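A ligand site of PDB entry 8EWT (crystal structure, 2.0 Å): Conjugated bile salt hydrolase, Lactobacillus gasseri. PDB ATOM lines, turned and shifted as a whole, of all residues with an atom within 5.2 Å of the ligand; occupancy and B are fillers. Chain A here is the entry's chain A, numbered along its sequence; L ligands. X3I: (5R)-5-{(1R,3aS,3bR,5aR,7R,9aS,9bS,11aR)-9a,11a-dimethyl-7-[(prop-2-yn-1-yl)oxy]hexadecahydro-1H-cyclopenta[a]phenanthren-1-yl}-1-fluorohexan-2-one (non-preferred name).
N of Cys 2 lies within hydrogen-bond range of OD1 of Asn 174 (3.3 Å).
The backbone NH (N) of Gly 79 sits at hydrogen-bond distance from the backbone carbonyl oxygen (O) of Phe 67 (3.1 Å).
The guanidinium group (NH1) of Arg 18 sits at hydrogen-bond distance from the backbone carbonyl oxygen (O) of Phe 67 (3.1 Å).
NH2 of Arg 18 lies within hydrogen-bond range of O of Gly 79 (2.8 Å).
The side-chain amide nitrogen (ND2) of Asn 174 sits at hydrogen-bond distance from the backbone carbonyl oxygen (O) of Asn 81 (2.9 Å).
NH2 of Arg 18 is in hydrogen-bond range of SG of Cys 2 (3.3 Å).
The backbone carbonyl oxygen of Ile 58 is in hydrogen-bond range of the backbone NH of Ser 65.
N of Cys 2 is in hydrogen-bond range of OD2 of Asp 21 (3.0 Å).
Residues that only touch the ligand: Asp 21 (3.1 Å), Tyr 26 (3.7 Å), Ile 58 (3.8 Å), Ser 65 (3.9 Å), Tyr 66 (3.9 Å), Phe 67 (3.6 Å), Gly 79 (3.7 Å), Leu 80 (3.7 Å), Tyr 102 (3.9 Å), Ile 132 (3.5 Å), Phe 136 (3.6 Å) and Ala 137 (3.5 Å).
Hydrophobic or aromatic side chains within 4 Å of the ligand: Tyr 26, Ile 58, Phe 67, Leu 80, Tyr 102 and Phe 136.
Of the 23 residues printed, 15 come within 4 Å of the ligand.
The nearest printed residue that does not touch the ligand is Val 22 (4.01 Å).
An oxygen (O28) of the ligand lies within hydrogen-bond range of the side-chain amide nitrogen (ND2) of Asn 174.
SG of Cys 2 is covalently linked to C27 of the ligand (1.8 Å).
The backbone NH of Asn 81 sits at hydrogen-bond distance from an oxygen (O28) of the ligand (2.7 Å).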
ATOM      1  N   CYS A   2      28.191 -11.218  31.062  1.00  0.00           N
ATOM      2  CA  CYS A   2      28.776 -12.208  30.147  1.00  0.00           C
ATOM      3  C   CYS A   2      30.178 -12.566  30.582  1.00  0.00           C
ATOM      4  O   CYS A   2      30.912 -11.723  31.097  1.00  0.00           O
ATOM      5  CB  CYS A   2      28.825 -11.696  28.714  1.00  0.00           C
ATOM      6  SG  CYS A   2      27.246 -11.609  27.905  1.00  0.00           S
ATOM      7  N   ARG A  18      31.063 -18.840  25.609  1.00  0.00           N
ATOM      8  CA  ARG A  18      30.664 -17.724  26.475  1.00  0.00           C
ATOM      9  C   ARG A  18      29.327 -17.992  27.136  1.00  0.00           C
ATOM     10  O   ARG A  18      28.502 -18.774  26.654  1.00  0.00           O
ATOM     11  CB  ARG A  18      30.582 -16.388  25.709  1.00  0.00           C
ATOM     12  CG  ARG A  18      29.594 -16.346  24.516  1.00  0.00           C
ATOM     13  CD  ARG A  18      28.147 -15.877  24.882  1.00  0.00           C
ATOM     14  NE  ARG A  18      28.074 -14.462  25.244  1.00  0.00           N
ATOM     15  CZ  ARG A  18      28.273 -13.459  24.399  1.00  0.00           C
ATOM     16  NH1 ARG A  18      28.449 -13.663  23.104  1.00  0.00           N
ATOM     17  NH2 ARG A  18      28.324 -12.215  24.877  1.00  0.00           N
ATOM     18  N   ASN A  19      29.108 -17.298  28.258  1.00  0.00           N
ATOM     19  CA  ASN A  19      27.790 -17.075  28.825  1.00  0.00           C
ATOM     20  C   ASN A  19      27.215 -15.786  28.256  1.00  0.00           C
ATOM     21  O   ASN A  19      27.938 -14.796  28.113  1.00  0.00           O
ATOM     22  CB  ASN A  19      27.844 -16.941  30.356  1.00  0.00           C
ATOM     23  CG  ASN A  19      28.032 -18.263  31.086  1.00  0.00           C
ATOM     24  OD1 ASN A  19      27.723 -19.358  30.587  1.00  0.00           O
ATOM     25  ND2 ASN A  19      28.539 -18.168  32.319  1.00  0.00           N
ATOM     26  N   LEU A  20      25.901 -15.783  27.969  1.00  0.00           N
ATOM     27  CA  LEU A  20      25.156 -14.573  27.626  1.00  0.00           C
ATOM     28  C   LEU A  20      24.264 -14.187  28.804  1.00  0.00           C
ATOM     29  O   LEU A  20      23.247 -14.847  29.054  1.00  0.00           O
ATOM     30  CB  LEU A  20      24.313 -14.762  26.355  1.00  0.00           C
ATOM     31  CG  LEU A  20      23.693 -13.426  25.885  1.00  0.00           C
ATOM     32  CD1 LEU A  20      24.746 -12.576  25.228  1.00  0.00           C
ATOM     33  CD2 LEU A  20      22.454 -13.555  24.982  1.00  0.00           C
ATOM     34  N   ASP A  21      24.631 -13.107  29.501  1.00  0.00           N
ATOM     35  CA  ASP A  21      23.892 -12.613  30.665  1.00  0.00           C
ATOM     36  C   ASP A  21      23.195 -11.308  30.274  1.00  0.00           C
ATOM     37  O   ASP A  21      23.851 -10.273  30.166  1.00  0.00           O
ATOM     38  CB  ASP A  21      24.812 -12.393  31.857  1.00  0.00           C
ATOM     39  CG  ASP A  21      25.779 -13.560  32.100  1.00  0.00           C
ATOM     40  OD1 ASP A  21      25.503 -14.691  31.643  1.00  0.00           O
ATOM     41  OD2 ASP A  21      26.819 -13.352  32.751  1.00  0.00           O
ATOM     42  N   VAL A  22      21.873 -11.362  30.063  1.00  0.00           N
ATOM     43  CA  VAL A  22      21.120 -10.209  29.573  1.00  0.00           C
ATOM     44  C   VAL A  22      19.849 -10.027  30.386  1.00  0.00           C
ATOM     45  O   VAL A  22      19.468 -10.885  31.197  1.00  0.00           O
ATOM     46  CB  VAL A  22      20.792 -10.334  28.069  1.00  0.00           C
ATOM     47  CG1 VAL A  22      22.040 -10.028  27.247  1.00  0.00           C
ATOM     48  CG2 VAL A  22      20.279 -11.709  27.766  1.00  0.00           C
ATOM     49  N   TYR A  26      16.319 -11.103  22.742  1.00  0.00           N
ATOM     50  CA  TYR A  26      16.802 -10.563  21.487  1.00  0.00           C
ATOM     51  C   TYR A  26      16.424 -11.398  20.270  1.00  0.00           C
ATOM     52  O   TYR A  26      16.791 -11.033  19.149  1.00  0.00           O
ATOM     53  CB  TYR A  26      18.327 -10.414  21.508  1.00  0.00           C
ATOM     54  CG  TYR A  26      18.831  -9.387  22.482  1.00  0.00           C
ATOM     55  CD1 TYR A  26      18.974  -8.056  22.108  1.00  0.00           C
ATOM     56  CD2 TYR A  26      19.170  -9.743  23.783  1.00  0.00           C
ATOM     57  CE1 TYR A  26      19.431  -7.098  23.010  1.00  0.00           C
ATOM     58  CE2 TYR A  26      19.626  -8.785  24.695  1.00  0.00           C
ATOM     59  CZ  TYR A  26      19.756  -7.478  24.298  1.00  0.00           C
ATOM     60  OH  TYR A  26      20.219  -6.538  25.190  1.00  0.00           O
ATOM     61  N   ILE A  58      21.288 -13.133  15.327  1.00  0.00           N
ATOM     62  CA  ILE A  58      20.049 -12.870  14.613  1.00  0.00           C
ATOM     63  C   ILE A  58      20.383 -12.601  13.148  1.00  0.00           C
ATOM     64  O   ILE A  58      21.521 -12.278  12.789  1.00  0.00           O
ATOM     65  CB  ILE A  58      19.260 -11.699  15.232  1.00  0.00           C
ATOM     66  CG1 ILE A  58      20.075 -10.414  15.141  1.00  0.00           C
ATOM     67  CG2 ILE A  58      18.864 -12.002  16.676  1.00  0.00           C
ATOM     68  CD1 ILE A  58      19.291  -9.178  15.472  1.00  0.00           C
ATOM     69  N   SER A  65      24.003 -11.542  12.002  1.00  0.00           N
ATOM     70  CA  SER A  65      24.620 -10.674  13.009  1.00  0.00           C
ATOM     71  C   SER A  65      24.905 -11.503  14.260  1.00  0.00           C
ATOM     72  O   SER A  65      24.017 -11.788  15.058  1.00  0.00           O
ATOM     73  CB  SER A  65      23.696  -9.501  13.338  1.00  0.00           C
ATOM     74  OG  SER A  65      22.955  -9.149  12.178  1.00  0.00           O
ATOM     75  N   TYR A  66      26.159 -11.874  14.443  1.00  0.00           N
ATOM     76  CA  TYR A  66      26.524 -12.858  15.441  1.00  0.00           C
ATOM     77  C   TYR A  66      26.811 -12.213  16.795  1.00  0.00           C
ATOM     78  O   TYR A  66      27.424 -11.144  16.866  1.00  0.00           O
ATOM     79  CB  TYR A  66      27.743 -13.642  14.984  1.00  0.00           C
ATOM     80  CG  TYR A  66      27.440 -14.726  13.991  1.00  0.00           C
ATOM     81  CD1 TYR A  66      26.846 -15.914  14.410  1.00  0.00           C
ATOM     82  CD2 TYR A  66      27.765 -14.587  12.648  1.00  0.00           C
ATOM     83  CE1 TYR A  66      26.575 -16.934  13.526  1.00  0.00           C
ATOM     84  CE2 TYR A  66      27.499 -15.615  11.744  1.00  0.00           C
ATOM     85  CZ  TYR A  66      26.897 -16.785  12.193  1.00  0.00           C
ATOM     86  OH  TYR A  66      26.636 -17.814  11.321  1.00  0.00           O
ATOM     87  N   PHE A  67      26.363 -12.893  17.873  1.00  0.00           N
ATOM     88  CA  PHE A  67      26.822 -12.609  19.234  1.00  0.00           C
ATOM     89  C   PHE A  67      28.198 -13.242  19.475  1.00  0.00           C
ATOM     90  O   PHE A  67      29.019 -12.708  20.222  1.00  0.00           O
ATOM     91  CB  PHE A  67      25.834 -13.163  20.283  1.00  0.00           C
ATOM     92  CG  PHE A  67      24.428 -12.605  20.215  1.00  0.00           C
ATOM     93  CD1 PHE A  67      23.971 -11.854  19.139  1.00  0.00           C
ATOM     94  CD2 PHE A  67      23.533 -12.871  21.256  1.00  0.00           C
ATOM     95  CE1 PHE A  67      22.670 -11.366  19.100  1.00  0.00           C
ATOM     96  CE2 PHE A  67      22.222 -12.386  21.225  1.00  0.00           C
ATOM     97  CZ  PHE A  67      21.793 -11.628  20.153  1.00  0.00           C
ATOM     98  N   GLY A  79      31.468 -11.114  21.107  1.00  0.00           N
ATOM     99  CA  GLY A  79      31.213  -9.752  21.523  1.00  0.00           C
ATOM    100  C   GLY A  79      30.555  -9.711  22.898  1.00  0.00           C
ATOM    101  O   GLY A  79      29.589 -10.423  23.161  1.00  0.00           O
ATOM    102  N   LEU A  80      31.114  -8.872  23.774  1.00  0.00           N
ATOM    103  CA  LEU A  80      30.617  -8.702  25.128  1.00  0.00           C
ATOM    104  C   LEU A  80      30.464  -7.210  25.425  1.00  0.00           C
ATOM    105  O   LEU A  80      31.193  -6.376  24.888  1.00  0.00           O
ATOM    106  CB  LEU A  80      31.560  -9.332  26.163  1.00  0.00           C
ATOM    107  CG  LEU A  80      31.504 -10.851  26.363  1.00  0.00           C
ATOM    108  CD1 LEU A  80      32.018 -11.597  25.133  1.00  0.00           C
ATOM    109  CD2 LEU A  80      32.299 -11.266  27.596  1.00  0.00           C
ATOM    110  N   ASN A  81      29.533  -6.892  26.320  1.00  0.00           N
ATOM    111  CA  ASN A  81      29.243  -5.504  26.653  1.00  0.00           C
ATOM    112  C   ASN A  81      30.432  -4.812  27.326  1.00  0.00           C
ATOM    113  O   ASN A  81      31.094  -5.376  28.198  1.00  0.00           O
ATOM    114  CB  ASN A  81      28.014  -5.451  27.582  1.00  0.00           C
ATOM    115  CG  ASN A  81      26.983  -4.424  27.140  1.00  0.00           C
ATOM    116  OD1 ASN A  81      26.856  -4.117  25.953  1.00  0.00           O
ATOM    117  ND2 ASN A  81      26.243  -3.892  28.104  1.00  0.00           N
ATOM    118  N   TYR A 102      29.743  -3.634  14.146  1.00  0.00           N
ATOM    119  CA  TYR A 102      29.073  -4.930  14.032  1.00  0.00           C
ATOM    120  C   TYR A 102      29.699  -5.822  12.968  1.00  0.00           C
ATOM    121  O   TYR A 102      29.576  -7.054  13.048  1.00  0.00           O
ATOM    122  CB  TYR A 102      27.571  -4.745  13.764  1.00  0.00           C
ATOM    123  CG  TYR A 102      27.211  -4.317  12.355  1.00  0.00           C
ATOM    124  CD1 TYR A 102      27.121  -2.979  12.012  1.00  0.00           C
ATOM    125  CD2 TYR A 102      26.940  -5.260  11.355  1.00  0.00           C
ATOM    126  CE1 TYR A 102      26.801  -2.578  10.727  1.00  0.00           C
ATOM    127  CE2 TYR A 102      26.614  -4.881  10.078  1.00  0.00           C
ATOM    128  CZ  TYR A 102      26.546  -3.529   9.769  1.00  0.00           C
ATOM    129  OH  TYR A 102      26.223  -3.119   8.494  1.00  0.00           O
ATOM    130  N   ALA A 131      25.374   1.897  12.829  1.00  0.00           N
ATOM    131  CA  ALA A 131      24.532   0.733  13.066  1.00  0.00           C
ATOM    132  C   ALA A 131      24.235   0.012  11.756  1.00  0.00           C
ATOM    133  O   ALA A 131      24.523   0.492  10.653  1.00  0.00           O
ATOM    134  CB  ALA A 131      23.230   1.139  13.748  1.00  0.00           C
ATOM    135  N   ILE A 132      23.643  -1.183  11.881  1.00  0.00           N
ATOM    136  CA  ILE A 132      23.321  -1.956  10.685  1.00  0.00           C
ATOM    137  C   ILE A 132      22.193  -1.306   9.901  1.00  0.00           C
ATOM    138  O   ILE A 132      22.212  -1.261   8.674  1.00  0.00           O
ATOM    139  CB  ILE A 132      23.031  -3.422  11.071  1.00  0.00           C
ATOM    140  CG1 ILE A 132      23.208  -4.348   9.867  1.00  0.00           C
ATOM    141  CG2 ILE A 132      21.660  -3.585  11.736  1.00  0.00           C
ATOM    142  CD1 ILE A 132      23.026  -5.828  10.165  1.00  0.00           C
ATOM    143  N   PHE A 136      18.367  -0.475  14.831  1.00  0.00           N
ATOM    144  CA  PHE A 136      19.250  -0.975  15.867  1.00  0.00           C
ATOM    145  C   PHE A 136      20.190   0.130  16.346  1.00  0.00           C
ATOM    146  O   PHE A 136      20.609   0.986  15.559  1.00  0.00           O
ATOM    147  CB  PHE A 136      20.068  -2.166  15.372  1.00  0.00           C
ATOM    148  CG  PHE A 136      19.242  -3.375  15.052  1.00  0.00           C
ATOM    149  CD1 PHE A 136      18.667  -3.525  13.797  1.00  0.00           C
ATOM    150  CD2 PHE A 136      19.034  -4.354  15.998  1.00  0.00           C
ATOM    151  CE1 PHE A 136      17.899  -4.630  13.492  1.00  0.00           C
ATOM    152  CE2 PHE A 136      18.267  -5.469  15.703  1.00  0.00           C
ATOM    153  CZ  PHE A 136      17.700  -5.607  14.449  1.00  0.00           C
ATOM    154  N   ALA A 137      20.519   0.111  17.629  1.00  0.00           N
ATOM    155  CA  ALA A 137      21.539   1.017  18.144  1.00  0.00           C
ATOM    156  C   ALA A 137      22.897   0.320  18.105  1.00  0.00           C
ATOM    157  O   ALA A 137      22.996  -0.908  18.072  1.00  0.00           O
ATOM    158  CB  ALA A 137      21.199   1.467  19.557  1.00  0.00           C
ATOM    159  N   VAL A 138      23.951   1.134  18.082  1.00  0.00           N
ATOM    160  CA  VAL A 138      25.303   0.588  18.073  1.00  0.00           C
ATOM    161  C   VAL A 138      25.596   0.012  19.454  1.00  0.00           C
ATOM    162  O   VAL A 138      25.486   0.705  20.469  1.00  0.00           O
ATOM    163  CB  VAL A 138      26.325   1.656  17.660  1.00  0.00           C
ATOM    164  CG1 VAL A 138      27.755   1.207  17.971  1.00  0.00           C
ATOM    165  CG2 VAL A 138      26.191   1.954  16.169  1.00  0.00           C
ATOM    166  N   ALA A 139      25.939  -1.257  19.510  1.00  0.00           N
ATOM    167  CA  ALA A 139      26.170  -1.904  20.787  1.00  0.00           C
ATOM    168  C   ALA A 139      27.574  -1.556  21.282  1.00  0.00           C
ATOM    169  O   ALA A 139      28.521  -1.596  20.489  1.00  0.00           O
ATOM    170  CB  ALA A 139      26.012  -3.412  20.662  1.00  0.00           C
ATOM    171  N   LEU A 141      30.468  -2.695  22.467  1.00  0.00           N
ATOM    172  CA  LEU A 141      31.106  -3.986  22.669  1.00  0.00           C
ATOM    173  C   LEU A 141      32.613  -3.877  22.806  1.00  0.00           C
ATOM    174  O   LEU A 141      33.246  -2.924  22.326  1.00  0.00           O
ATOM    175  CB  LEU A 141      30.766  -4.938  21.509  1.00  0.00           C
ATOM    176  CG  LEU A 141      29.298  -5.228  21.233  1.00  0.00           C
ATOM    177  CD1 LEU A 141      29.187  -6.263  20.116  1.00  0.00           C
ATOM    178  CD2 LEU A 141      28.613  -5.701  22.498  1.00  0.00           C
ATOM    179  N   ASN A 174      33.047  -7.894  31.533  1.00  0.00           N
ATOM    180  CA  ASN A 174      32.562  -6.591  31.108  1.00  0.00           C
ATOM    181  C   ASN A 174      33.422  -5.477  31.698  1.00  0.00           C
ATOM    182  O   ASN A 174      34.588  -5.719  32.020  1.00  0.00           O
ATOM    183  CB  ASN A 174      31.076  -6.429  31.497  1.00  0.00           C
ATOM    184  CG  ASN A 174      30.213  -7.578  30.985  1.00  0.00           C
ATOM    185  OD1 ASN A 174      29.835  -8.464  31.744  1.00  0.00           O
ATOM    186  ND2 ASN A 174      29.924  -7.589  29.685  1.00  0.00           N
HETATM  187  C13 X3I L   1      21.873  -5.526  17.922  1.00  0.00           C
HETATM  188  C15 X3I L   1      21.458  -7.934  18.318  1.00  0.00           C
HETATM  189  C17 X3I L   1      22.600  -6.452  20.727  1.00  0.00           C
HETATM  190  C20 X3I L   1      23.063  -8.971  22.388  1.00  0.00           C
HETATM  191  C21 X3I L   1      25.157  -7.933  23.361  1.00  0.00           C
HETATM  192  C22 X3I L   1      24.704  -8.085  24.829  1.00  0.00           C
HETATM  193  C24 X3I L   1      25.949  -8.373  25.683  1.00  0.00           C
HETATM  194  C26 X3I L   1      26.874  -8.933  27.903  1.00  0.00           C
HETATM  195  C01 X3I L   1      25.005  -8.064  20.989  1.00  0.00           C
HETATM  196  C02 X3I L   1      24.224  -8.136  19.683  1.00  0.00           C
HETATM  197  C03 X3I L   1      25.110  -8.430  18.481  1.00  0.00           C
HETATM  198  C04 X3I L   1      24.301  -8.477  17.183  1.00  0.00           C
HETATM  199  C05 X3I L   1      23.516  -7.178  16.983  1.00  0.00           C
HETATM  200  C06 X3I L   1      24.463  -6.018  16.668  1.00  0.00           C
HETATM  201  C07 X3I L   1      23.685  -4.746  16.396  1.00  0.00           C
HETATM  202  C09 X3I L   1      23.943  -2.822  14.936  1.00  0.00           C
HETATM  203  C12 X3I L   1      22.824  -4.374  17.586  1.00  0.00           C
HETATM  204  C14 X3I L   1      22.568  -6.878  18.178  1.00  0.00           C
HETATM  205  C16 X3I L   1      23.427  -6.830  19.482  1.00  0.00           C
HETATM  206  C18 X3I L   1      23.426  -6.483  22.021  1.00  0.00           C
HETATM  207  C19 X3I L   1      24.100  -7.848  22.223  1.00  0.00           C
HETATM  208  C23 X3I L   1      23.948  -6.861  25.344  1.00  0.00           C
HETATM  209  C25 X3I L   1      25.691  -8.361  27.197  1.00  0.00           C
HETATM  210  C27 X3I L   1      26.552 -10.166  28.665  1.00  0.00           C
HETATM  211  C29 X3I L   1      26.096  -9.087  22.904  1.00  0.00           C
HETATM  212  C30 X3I L   1      25.893  -9.244  21.372  1.00  0.00           C
HETATM  213  O08 X3I L   1      24.513  -3.628  15.962  1.00  0.00           O
HETATM  214  O28 X3I L   1      28.018  -8.527  27.813  1.00  0.00           O
